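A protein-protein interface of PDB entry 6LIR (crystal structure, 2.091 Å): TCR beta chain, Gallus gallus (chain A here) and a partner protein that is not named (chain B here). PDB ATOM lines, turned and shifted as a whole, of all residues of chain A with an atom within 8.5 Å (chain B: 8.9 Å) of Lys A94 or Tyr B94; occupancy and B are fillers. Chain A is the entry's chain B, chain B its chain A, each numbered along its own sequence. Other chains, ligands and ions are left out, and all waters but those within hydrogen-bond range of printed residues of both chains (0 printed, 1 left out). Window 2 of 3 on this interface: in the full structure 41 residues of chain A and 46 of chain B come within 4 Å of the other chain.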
ATOM      1  N   HIS A  26      20.262  10.760   4.451  1.00  0.00           N
ATOM      2  CA  HIS A  26      20.915   9.741   3.645  1.00  0.00           C
ATOM      3  C   HIS A  26      19.997   8.547   3.455  1.00  0.00           C
ATOM      4  O   HIS A  26      19.351   8.089   4.401  1.00  0.00           O
ATOM      5  CB  HIS A  26      22.216   9.289   4.306  1.00  0.00           C
ATOM      6  CG  HIS A  26      23.372  10.201   4.051  1.00  0.00           C
ATOM      7  ND1 HIS A  26      24.597  10.034   4.658  1.00  0.00           N
ATOM      8  CD2 HIS A  26      23.489  11.291   3.258  1.00  0.00           C
ATOM      9  CE1 HIS A  26      25.421  10.982   4.247  1.00  0.00           C
ATOM     10  NE2 HIS A  26      24.773  11.758   3.397  1.00  0.00           N
ATOM     11  N   ASP A  27      19.956   8.025   2.229  1.00  0.00           N
ATOM     12  CA  ASP A  27      19.122   6.856   1.982  1.00  0.00           C
ATOM     13  C   ASP A  27      19.810   5.573   2.422  1.00  0.00           C
ATOM     14  O   ASP A  27      19.143   4.648   2.897  1.00  0.00           O
ATOM     15  CB  ASP A  27      18.766   6.759   0.495  1.00  0.00           C
ATOM     16  CG  ASP A  27      17.898   7.911   0.021  1.00  0.00           C
ATOM     17  OD1 ASP A  27      17.193   8.517   0.858  1.00  0.00           O
ATOM     18  OD2 ASP A  27      17.923   8.209  -1.193  1.00  0.00           O
ATOM     19  N   TYR A  28      21.134   5.505   2.307  1.00  0.00           N
ATOM     20  CA  TYR A  28      21.869   4.305   2.675  1.00  0.00           C
ATOM     21  C   TYR A  28      22.341   4.414   4.116  1.00  0.00           C
ATOM     22  O   TYR A  28      22.917   5.431   4.515  1.00  0.00           O
ATOM     23  CB  TYR A  28      23.064   4.089   1.744  1.00  0.00           C
ATOM     24  CG  TYR A  28      23.797   2.788   1.985  1.00  0.00           C
ATOM     25  CD1 TYR A  28      23.339   1.596   1.432  1.00  0.00           C
ATOM     26  CD2 TYR A  28      24.947   2.748   2.766  1.00  0.00           C
ATOM     27  CE1 TYR A  28      24.005   0.405   1.650  1.00  0.00           C
ATOM     28  CE2 TYR A  28      25.619   1.562   2.990  1.00  0.00           C
ATOM     29  CZ  TYR A  28      25.144   0.393   2.429  1.00  0.00           C
ATOM     30  OH  TYR A  28      25.810  -0.793   2.647  1.00  0.00           O
ATOM     31  N   MET A  29      22.082   3.367   4.895  1.00  0.00           N
ATOM     32  CA  MET A  29      22.660   3.223   6.219  1.00  0.00           C
ATOM     33  C   MET A  29      23.140   1.790   6.364  1.00  0.00           C
ATOM     34  O   MET A  29      22.698   0.894   5.642  1.00  0.00           O
ATOM     35  CB  MET A  29      21.656   3.577   7.323  1.00  0.00           C
ATOM     36  CG  MET A  29      21.149   5.000   7.241  1.00  0.00           C
ATOM     37  SD  MET A  29      20.094   5.412   8.633  1.00  0.00           S
ATOM     38  CE  MET A  29      21.280   5.334   9.978  1.00  0.00           C
ATOM     39  N   SER A  30      24.033   1.570   7.323  1.00  0.00           N
ATOM     40  CA  SER A  30      24.598   0.238   7.464  1.00  0.00           C
ATOM     41  C   SER A  30      25.158   0.070   8.863  1.00  0.00           C
ATOM     42  O   SER A  30      25.415   1.044   9.574  1.00  0.00           O
ATOM     43  CB  SER A  30      25.686  -0.016   6.416  1.00  0.00           C
ATOM     44  OG  SER A  30      26.741   0.918   6.553  1.00  0.00           O
ATOM     45  N   TYR A  32      28.283  -2.177  10.838  1.00  0.00           N
ATOM     46  CA  TYR A  32      29.538  -2.865  10.578  1.00  0.00           C
ATOM     47  C   TYR A  32      30.082  -3.412  11.885  1.00  0.00           C
ATOM     48  O   TYR A  32      29.858  -2.841  12.956  1.00  0.00           O
ATOM     49  CB  TYR A  32      30.579  -1.927   9.947  1.00  0.00           C
ATOM     50  CG  TYR A  32      30.456  -1.775   8.451  1.00  0.00           C
ATOM     51  CD1 TYR A  32      31.075  -2.675   7.593  1.00  0.00           C
ATOM     52  CD2 TYR A  32      29.724  -0.731   7.893  1.00  0.00           C
ATOM     53  CE1 TYR A  32      30.966  -2.546   6.221  1.00  0.00           C
ATOM     54  CE2 TYR A  32      29.611  -0.593   6.516  1.00  0.00           C
ATOM     55  CZ  TYR A  32      30.238  -1.504   5.687  1.00  0.00           C
ATOM     56  OH  TYR A  32      30.137  -1.388   4.320  1.00  0.00           O
ATOM     57  N   LEU A  42      30.266  -6.044   7.151  1.00  0.00           N
ATOM     58  CA  LEU A  42      28.875  -5.613   7.076  1.00  0.00           C
ATOM     59  C   LEU A  42      27.945  -6.618   7.748  1.00  0.00           C
ATOM     60  O   LEU A  42      27.875  -7.784   7.343  1.00  0.00           O
ATOM     61  CB  LEU A  42      28.458  -5.385   5.628  1.00  0.00           C
ATOM     62  CG  LEU A  42      27.106  -4.671   5.541  1.00  0.00           C
ATOM     63  CD1 LEU A  42      27.287  -3.167   5.640  1.00  0.00           C
ATOM     64  CD2 LEU A  42      26.375  -5.041   4.261  1.00  0.00           C
ATOM     65  N   SER A  45      22.552  -3.810   6.146  1.00  0.00           N
ATOM     66  CA  SER A  45      22.491  -2.527   5.464  1.00  0.00           C
ATOM     67  C   SER A  45      21.041  -2.215   5.125  1.00  0.00           C
ATOM     68  O   SER A  45      20.145  -3.043   5.307  1.00  0.00           O
ATOM     69  CB  SER A  45      23.353  -2.522   4.194  1.00  0.00           C
ATOM     70  OG  SER A  45      22.780  -3.341   3.186  1.00  0.00           O
ATOM     71  N   SER A  46      20.823  -1.015   4.594  1.00  0.00           N
ATOM     72  CA  SER A  46      19.483  -0.555   4.263  1.00  0.00           C
ATOM     73  C   SER A  46      19.588   0.455   3.135  1.00  0.00           C
ATOM     74  O   SER A  46      20.332   1.434   3.249  1.00  0.00           O
ATOM     75  CB  SER A  46      18.804   0.085   5.482  1.00  0.00           C
ATOM     76  OG  SER A  46      17.603   0.744   5.111  1.00  0.00           O
ATOM     77  N   TYR A  47      18.837   0.231   2.061  1.00  0.00           N
ATOM     78  CA  TYR A  47      18.840   1.152   0.935  1.00  0.00           C
ATOM     79  C   TYR A  47      17.774   2.228   1.062  1.00  0.00           C
ATOM     80  O   TYR A  47      17.724   3.134   0.223  1.00  0.00           O
ATOM     81  CB  TYR A  47      18.641   0.392  -0.389  1.00  0.00           C
ATOM     82  CG  TYR A  47      19.672  -0.683  -0.680  1.00  0.00           C
ATOM     83  CD1 TYR A  47      20.985  -0.562  -0.237  1.00  0.00           C
ATOM     84  CD2 TYR A  47      19.332  -1.815  -1.415  1.00  0.00           C
ATOM     85  CE1 TYR A  47      21.928  -1.547  -0.510  1.00  0.00           C
ATOM     86  CE2 TYR A  47      20.266  -2.802  -1.691  1.00  0.00           C
ATOM     87  CZ  TYR A  47      21.562  -2.662  -1.235  1.00  0.00           C
ATOM     88  OH  TYR A  47      22.496  -3.639  -1.505  1.00  0.00           O
ATOM     89  N   ASN A  53      18.950  -5.359   4.281  1.00  0.00           N
ATOM     90  CA  ASN A  53      19.710  -6.390   3.586  1.00  0.00           C
ATOM     91  C   ASN A  53      20.643  -7.074   4.570  1.00  0.00           C
ATOM     92  O   ASN A  53      21.434  -6.406   5.246  1.00  0.00           O
ATOM     93  CB  ASN A  53      20.531  -5.806   2.430  1.00  0.00           C
ATOM     94  CG  ASN A  53      19.682  -5.060   1.427  1.00  0.00           C
ATOM     95  OD1 ASN A  53      18.898  -5.658   0.693  1.00  0.00           O
ATOM     96  ND2 ASN A  53      19.843  -3.743   1.381  1.00  0.00           N
ATOM     97  N   SER A  90      26.629   5.756   6.928  1.00  0.00           N
ATOM     98  CA  SER A  90      25.608   6.205   5.996  1.00  0.00           C
ATOM     99  C   SER A  90      26.257   6.803   4.757  1.00  0.00           C
ATOM    100  O   SER A  90      27.423   7.203   4.768  1.00  0.00           O
ATOM    101  CB  SER A  90      24.678   7.236   6.646  1.00  0.00           C
ATOM    102  OG  SER A  90      25.224   8.541   6.536  1.00  0.00           O
ATOM    103  N   SER A  91      25.470   6.870   3.684  1.00  0.00           N
ATOM    104  CA  SER A  91      25.849   7.593   2.482  1.00  0.00           C
ATOM    105  C   SER A  91      24.590   8.040   1.757  1.00  0.00           C
ATOM    106  O   SER A  91      23.492   7.533   2.007  1.00  0.00           O
ATOM    107  CB  SER A  91      26.730   6.743   1.562  1.00  0.00           C
ATOM    108  OG  SER A  91      26.083   5.529   1.231  1.00  0.00           O
ATOM    109  N   SER A  92      24.769   9.009   0.855  1.00  0.00           N
ATOM    110  CA  SER A  92      23.670   9.499   0.025  1.00  0.00           C
ATOM    111  C   SER A  92      22.948   8.350  -0.674  1.00  0.00           C
ATOM    112  O   SER A  92      21.712   8.280  -0.679  1.00  0.00           O
ATOM    113  CB  SER A  92      24.200  10.514  -0.987  1.00  0.00           C
ATOM    114  OG  SER A  92      23.410  10.538  -2.159  1.00  0.00           O
ATOM    115  N   TYR A  93      23.718   7.443  -1.270  1.00  0.00           N
ATOM    116  CA  TYR A  93      23.217   6.222  -1.886  1.00  0.00           C
ATOM    117  C   TYR A  93      24.401   5.273  -2.004  1.00  0.00           C
ATOM    118  O   TYR A  93      25.553   5.671  -1.813  1.00  0.00           O
ATOM    119  CB  TYR A  93      22.587   6.503  -3.259  1.00  0.00           C
ATOM    120  CG  TYR A  93      23.412   7.432  -4.136  1.00  0.00           C
ATOM    121  CD1 TYR A  93      24.621   7.015  -4.683  1.00  0.00           C
ATOM    122  CD2 TYR A  93      22.981   8.723  -4.419  1.00  0.00           C
ATOM    123  CE1 TYR A  93      25.380   7.857  -5.477  1.00  0.00           C
ATOM    124  CE2 TYR A  93      23.738   9.575  -5.212  1.00  0.00           C
ATOM    125  CZ  TYR A  93      24.935   9.136  -5.739  1.00  0.00           C
ATOM    126  OH  TYR A  93      25.691   9.973  -6.531  1.00  0.00           O
ATOM    127  N   LYS A  94      24.117   4.014  -2.319  1.00  0.00           N
ATOM    128  CA  LYS A  94      25.208   3.073  -2.511  1.00  0.00           C
ATOM    129  C   LYS A  94      25.857   3.275  -3.878  1.00  0.00           C
ATOM    130  O   LYS A  94      25.214   3.691  -4.846  1.00  0.00           O
ATOM    131  CB  LYS A  94      24.761   1.620  -2.342  1.00  0.00           C
ATOM    132  CG  LYS A  94      25.942   0.655  -2.477  1.00  0.00           C
ATOM    133  CD  LYS A  94      25.738  -0.664  -1.792  1.00  0.00           C
ATOM    134  CE  LYS A  94      25.232  -1.689  -2.773  1.00  0.00           C
ATOM    135  NZ  LYS A  94      25.262  -3.048  -2.189  1.00  0.00           N
ATOM    136  N   GLY A  95      27.144   2.950  -3.943  1.00  0.00           N
ATOM    137  CA  GLY A  95      27.943   3.007  -5.147  1.00  0.00           C
ATOM    138  C   GLY A  95      28.873   4.196  -5.212  1.00  0.00           C
ATOM    139  O   GLY A  95      28.463   5.320  -5.523  1.00  0.00           O
ATOM    140  N   ASN A  96      30.145   3.916  -4.938  1.00  0.00           N
ATOM    141  CA  ASN A  96      31.266   4.849  -5.048  1.00  0.00           C
ATOM    142  C   ASN A  96      30.905   6.245  -4.543  1.00  0.00           C
ATOM    143  O   ASN A  96      31.026   7.251  -5.243  1.00  0.00           O
ATOM    144  CB  ASN A  96      31.790   4.901  -6.481  1.00  0.00           C
ATOM    145  CG  ASN A  96      33.177   5.495  -6.561  1.00  0.00           C
ATOM    146  OD1 ASN A  96      33.816   5.743  -5.538  1.00  0.00           O
ATOM    147  ND2 ASN A  96      33.656   5.719  -7.778  1.00  0.00           N
ATOM    148  N   THR A  97      30.471   6.281  -3.285  1.00  0.00           N
ATOM    149  CA  THR A  97      30.096   7.501  -2.599  1.00  0.00           C
ATOM    150  C   THR A  97      30.628   7.302  -1.185  1.00  0.00           C
ATOM    151  O   THR A  97      30.430   6.222  -0.601  1.00  0.00           O
ATOM    152  CB  THR A  97      28.584   7.743  -2.584  1.00  0.00           C
ATOM    153  OG1 THR A  97      28.015   7.287  -3.819  1.00  0.00           O
ATOM    154  CG2 THR A  97      28.265   9.223  -2.404  1.00  0.00           C
ATOM    155  N   PRO A  98      31.315   8.289  -0.618  1.00  0.00           N
ATOM    156  CA  PRO A  98      31.935   8.085   0.695  1.00  0.00           C
ATOM    157  C   PRO A  98      30.901   7.724   1.754  1.00  0.00           C
ATOM    158  O   PRO A  98      29.779   8.238   1.763  1.00  0.00           O
ATOM    159  CB  PRO A  98      32.593   9.436   0.986  1.00  0.00           C
ATOM    160  CG  PRO A  98      31.803  10.413   0.170  1.00  0.00           C
ATOM    161  CD  PRO A  98      31.451   9.681  -1.082  1.00  0.00           C
ATOM    162  N   LEU A  99      31.297   6.835   2.654  1.00  0.00           N
ATOM    163  CA  LEU A  99      30.486   6.498   3.810  1.00  0.00           C
ATOM    164  C   LEU A  99      30.860   7.417   4.962  1.00  0.00           C
ATOM    165  O   LEU A  99      32.036   7.740   5.159  1.00  0.00           O
ATOM    166  CB  LEU A  99      30.698   5.040   4.223  1.00  0.00           C
ATOM    167  CG  LEU A  99      30.097   3.930   3.359  1.00  0.00           C
ATOM    168  CD1 LEU A  99      30.657   2.580   3.778  1.00  0.00           C
ATOM    169  CD2 LEU A  99      28.580   3.935   3.451  1.00  0.00           C
ATOM    170  N   TYR B  28      36.229  -2.086  -9.300  1.00  0.00           N
ATOM    171  CA  TYR B  28      35.570  -1.027 -10.052  1.00  0.00           C
ATOM    172  C   TYR B  28      35.950   0.333  -9.486  1.00  0.00           C
ATOM    173  O   TYR B  28      36.150   1.295 -10.236  1.00  0.00           O
ATOM    174  CB  TYR B  28      34.051  -1.210 -10.023  1.00  0.00           C
ATOM    175  CG  TYR B  28      33.291  -0.059 -10.649  1.00  0.00           C
ATOM    176  CD1 TYR B  28      33.073  -0.009 -12.021  1.00  0.00           C
ATOM    177  CD2 TYR B  28      32.800   0.984  -9.869  1.00  0.00           C
ATOM    178  CE1 TYR B  28      32.385   1.044 -12.599  1.00  0.00           C
ATOM    179  CE2 TYR B  28      32.111   2.041 -10.438  1.00  0.00           C
ATOM    180  CZ  TYR B  28      31.906   2.066 -11.802  1.00  0.00           C
ATOM    181  OH  TYR B  28      31.221   3.115 -12.370  1.00  0.00           O
ATOM    182  N   SER B  29      36.055   0.424  -8.166  1.00  0.00           N
ATOM    183  CA  SER B  29      36.469   1.649  -7.505  1.00  0.00           C
ATOM    184  C   SER B  29      37.170   1.272  -6.211  1.00  0.00           C
ATOM    185  O   SER B  29      36.895   0.226  -5.617  1.00  0.00           O
ATOM    186  CB  SER B  29      35.280   2.575  -7.221  1.00  0.00           C
ATOM    187  OG  SER B  29      34.462   2.046  -6.194  1.00  0.00           O
ATOM    188  N   GLN B  31      38.548   2.905  -2.424  1.00  0.00           N
ATOM    189  CA  GLN B  31      38.459   3.978  -1.454  1.00  0.00           C
ATOM    190  C   GLN B  31      39.391   3.664  -0.301  1.00  0.00           C
ATOM    191  O   GLN B  31      39.688   2.500  -0.016  1.00  0.00           O
ATOM    192  CB  GLN B  31      37.034   4.159  -0.913  1.00  0.00           C
ATOM    193  CG  GLN B  31      36.020   4.599  -1.947  1.00  0.00           C
ATOM    194  CD  GLN B  31      34.620   4.119  -1.621  1.00  0.00           C
ATOM    195  OE1 GLN B  31      33.949   3.522  -2.463  1.00  0.00           O
ATOM    196  NE2 GLN B  31      34.173   4.375  -0.395  1.00  0.00           N
ATOM    197  N   ARG B  90      35.400  -2.178  -4.505  1.00  0.00           N
ATOM    198  CA  ARG B  90      34.132  -2.615  -5.067  1.00  0.00           C
ATOM    199  C   ARG B  90      34.413  -3.344  -6.366  1.00  0.00           C
ATOM    200  O   ARG B  90      35.130  -2.827  -7.228  1.00  0.00           O
ATOM    201  CB  ARG B  90      33.175  -1.442  -5.303  1.00  0.00           C
ATOM    202  CG  ARG B  90      31.819  -1.631  -4.650  1.00  0.00           C
ATOM    203  CD  ARG B  90      30.854  -0.520  -5.028  1.00  0.00           C
ATOM    204  NE  ARG B  90      31.237   0.755  -4.433  1.00  0.00           N
ATOM    205  CZ  ARG B  90      30.859   1.157  -3.221  1.00  0.00           C
ATOM    206  NH1 ARG B  90      31.260   2.332  -2.755  1.00  0.00           N
ATOM    207  NH2 ARG B  90      30.086   0.380  -2.475  1.00  0.00           N
ATOM    208  N   GLY B  91      33.846  -4.544  -6.502  1.00  0.00           N
ATOM    209  CA  GLY B  91      34.045  -5.329  -7.707  1.00  0.00           C
ATOM    210  C   GLY B  91      33.257  -4.793  -8.884  1.00  0.00           C
ATOM    211  O   GLY B  91      33.616  -5.034 -10.039  1.00  0.00           O
ATOM    212  N   SER B  92      32.176  -4.070  -8.608  1.00  0.00           N
ATOM    213  CA  SER B  92      31.304  -3.523  -9.635  1.00  0.00           C
ATOM    214  C   SER B  92      30.648  -2.270  -9.081  1.00  0.00           C
ATOM    215  O   SER B  92      30.699  -2.004  -7.878  1.00  0.00           O
ATOM    216  CB  SER B  92      30.237  -4.527 -10.066  1.00  0.00           C
ATOM    217  OG  SER B  92      29.071  -4.365  -9.273  1.00  0.00           O
ATOM    218  N   SER B  93      30.066  -1.477  -9.983  1.00  0.00           N
ATOM    219  CA  SER B  93      29.324  -0.298  -9.550  1.00  0.00           C
ATOM    220  C   SER B  93      28.232  -0.665  -8.546  1.00  0.00           C
ATOM    221  O   SER B  93      28.008   0.058  -7.569  1.00  0.00           O
ATOM    222  CB  SER B  93      28.732   0.425 -10.766  1.00  0.00           C
ATOM    223  OG  SER B  93      28.098  -0.478 -11.655  1.00  0.00           O
ATOM    224  N   TYR B  94      27.555  -1.795  -8.763  1.00  0.00           N
ATOM    225  CA  TYR B  94      26.355  -2.146  -8.017  1.00  0.00           C
ATOM    226  C   TYR B  94      26.581  -3.094  -6.843  1.00  0.00           C
ATOM    227  O   TYR B  94      25.636  -3.335  -6.081  1.00  0.00           O
ATOM    228  CB  TYR B  94      25.314  -2.766  -8.966  1.00  0.00           C
ATOM    229  CG  TYR B  94      25.870  -3.771  -9.960  1.00  0.00           C
ATOM    230  CD1 TYR B  94      26.337  -3.365 -11.206  1.00  0.00           C
ATOM    231  CD2 TYR B  94      25.908  -5.128  -9.660  1.00  0.00           C
ATOM    232  CE1 TYR B  94      26.837  -4.281 -12.120  1.00  0.00           C
ATOM    233  CE2 TYR B  94      26.407  -6.051 -10.567  1.00  0.00           C
ATOM    234  CZ  TYR B  94      26.869  -5.622 -11.795  1.00  0.00           C
ATOM    235  OH  TYR B  94      27.365  -6.535 -12.699  1.00  0.00           O
ATOM    236  N   THR B  95      27.782  -3.639  -6.670  1.00  0.00           N
ATOM    237  CA  THR B  95      27.993  -4.711  -5.710  1.00  0.00           C
ATOM    238  C   THR B  95      28.579  -4.191  -4.401  1.00  0.00           C
ATOM    239  O   THR B  95      28.763  -2.994  -4.182  1.00  0.00           O
ATOM    240  CB  THR B  95      28.883  -5.820  -6.279  1.00  0.00           C
ATOM    241  OG1 THR B  95      29.987  -5.248  -6.993  1.00  0.00           O
ATOM    242  CG2 THR B  95      28.085  -6.732  -7.194  1.00  0.00           C
ATOM    243  N   LYS B  96      28.863  -5.135  -3.519  1.00  0.00           N
ATOM    244  CA  LYS B  96      29.250  -4.836  -2.153  1.00  0.00           C
ATOM    245  C   LYS B  96      30.622  -4.186  -2.045  1.00  0.00           C
ATOM    246  O   LYS B  96      31.552  -4.512  -2.788  1.00  0.00           O
ATOM    247  CB  LYS B  96      29.249  -6.121  -1.363  1.00  0.00           C
ATOM    248  CG  LYS B  96      29.172  -5.945   0.094  1.00  0.00           C
ATOM    249  CD  LYS B  96      29.786  -7.185   0.652  1.00  0.00           C
ATOM    250  CE  LYS B  96      28.954  -7.833   1.717  1.00  0.00           C
ATOM    251  NZ  LYS B  96      29.647  -9.098   2.152  1.00  0.00           N
ATOM    252  N   LEU B  97      30.735  -3.252  -1.103  1.00  0.00           N
ATOM    253  CA  LEU B  97      32.028  -2.718  -0.713  1.00  0.00           C
ATOM    254  C   LEU B  97      32.673  -3.695   0.261  1.00  0.00           C
ATOM    255  O   LEU B  97      32.025  -4.153   1.207  1.00  0.00           O
ATOM    256  CB  LEU B  97      31.845  -1.341  -0.074  1.00  0.00           C
ATOM    257  CG  LEU B  97      33.058  -0.454   0.195  1.00  0.00           C
ATOM    258  CD1 LEU B  97      33.608   0.103  -1.105  1.00  0.00           C
ATOM    259  CD2 LEU B  97      32.684   0.680   1.148  1.00  0.00           C
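The side-chain hydroxyl (OG) of Ser B92 sits at hydrogen-bond distance from the backbone NH (N) of Tyr B94 (3.0 Å).
The side-chain amide oxygen of Gln B31 lies within hydrogen-bond range of the guanidinium group of Arg B90 (3.0 Å).
O of Gly A95 sits at hydrogen-bond distance from OG1 of Thr A97, at 2.6 Å.
N of Arg B90 lies within hydrogen-bond range of O of Ser B29, at 3.0 Å.
OH of Tyr A47 is in hydrogen-bond range of NZ of Lys A94.
N of Tyr B28 lies within hydrogen-bond range of O of Arg B90 (2.5 Å).
Of the 21 printed residues of chain A, 4 touch a printed residue of chain B.
Hydrophobic or aromatic side chains of chain A that line the printed part of chain B: Leu A99.
Of the 11 printed residues of chain B, 6 touch a printed residue of chain A.
Among the printed residues, 7 pairs touch across the chains.
Among the printed residues, no Asp or Glu carboxylate lies within 4 Å of a Lys or Arg side-chain nitrogen of the other chain.
Among the printed residues, pairs that only touch across the chains: Asn A96 with Ser B29 (3.6 Å), Lys A94 with Tyr B94 (3.7 Å), Asn A96 with Gln B31 (3.8 Å), Gly A95 with Ser B93 (3.8 Å), Leu A99 with Leu B97 (3.8 Å) and Gly A95 with Arg B90 (3.9 Å).
Ser A91 touches none of the printed residues of chain B.
Of the printed residues of chain B, Lys A94 touches Tyr B94 (3.7 Å).
Of the printed residues of chain B, Asn A96 touches Ser B29 (3.6 Å), Gln B31 (3.8 Å) and Arg B90 (2.9 Å).
Printed residues of chain A within 4 Å of Arg B90: Gly A95 and Asn A96.
Of chain A, only Gly A95 (3.8 Å) comes within 4 Å of Ser B93.
Of chain A, only Lys A94 comes within 4 Å of Tyr B94.
The nearest printed residue of chain B that does not touch Lys A94 is Thr B95 (4.02 Å).
N of Asn A96 sits close to NH1 of Arg B90, 2.9 Å away.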
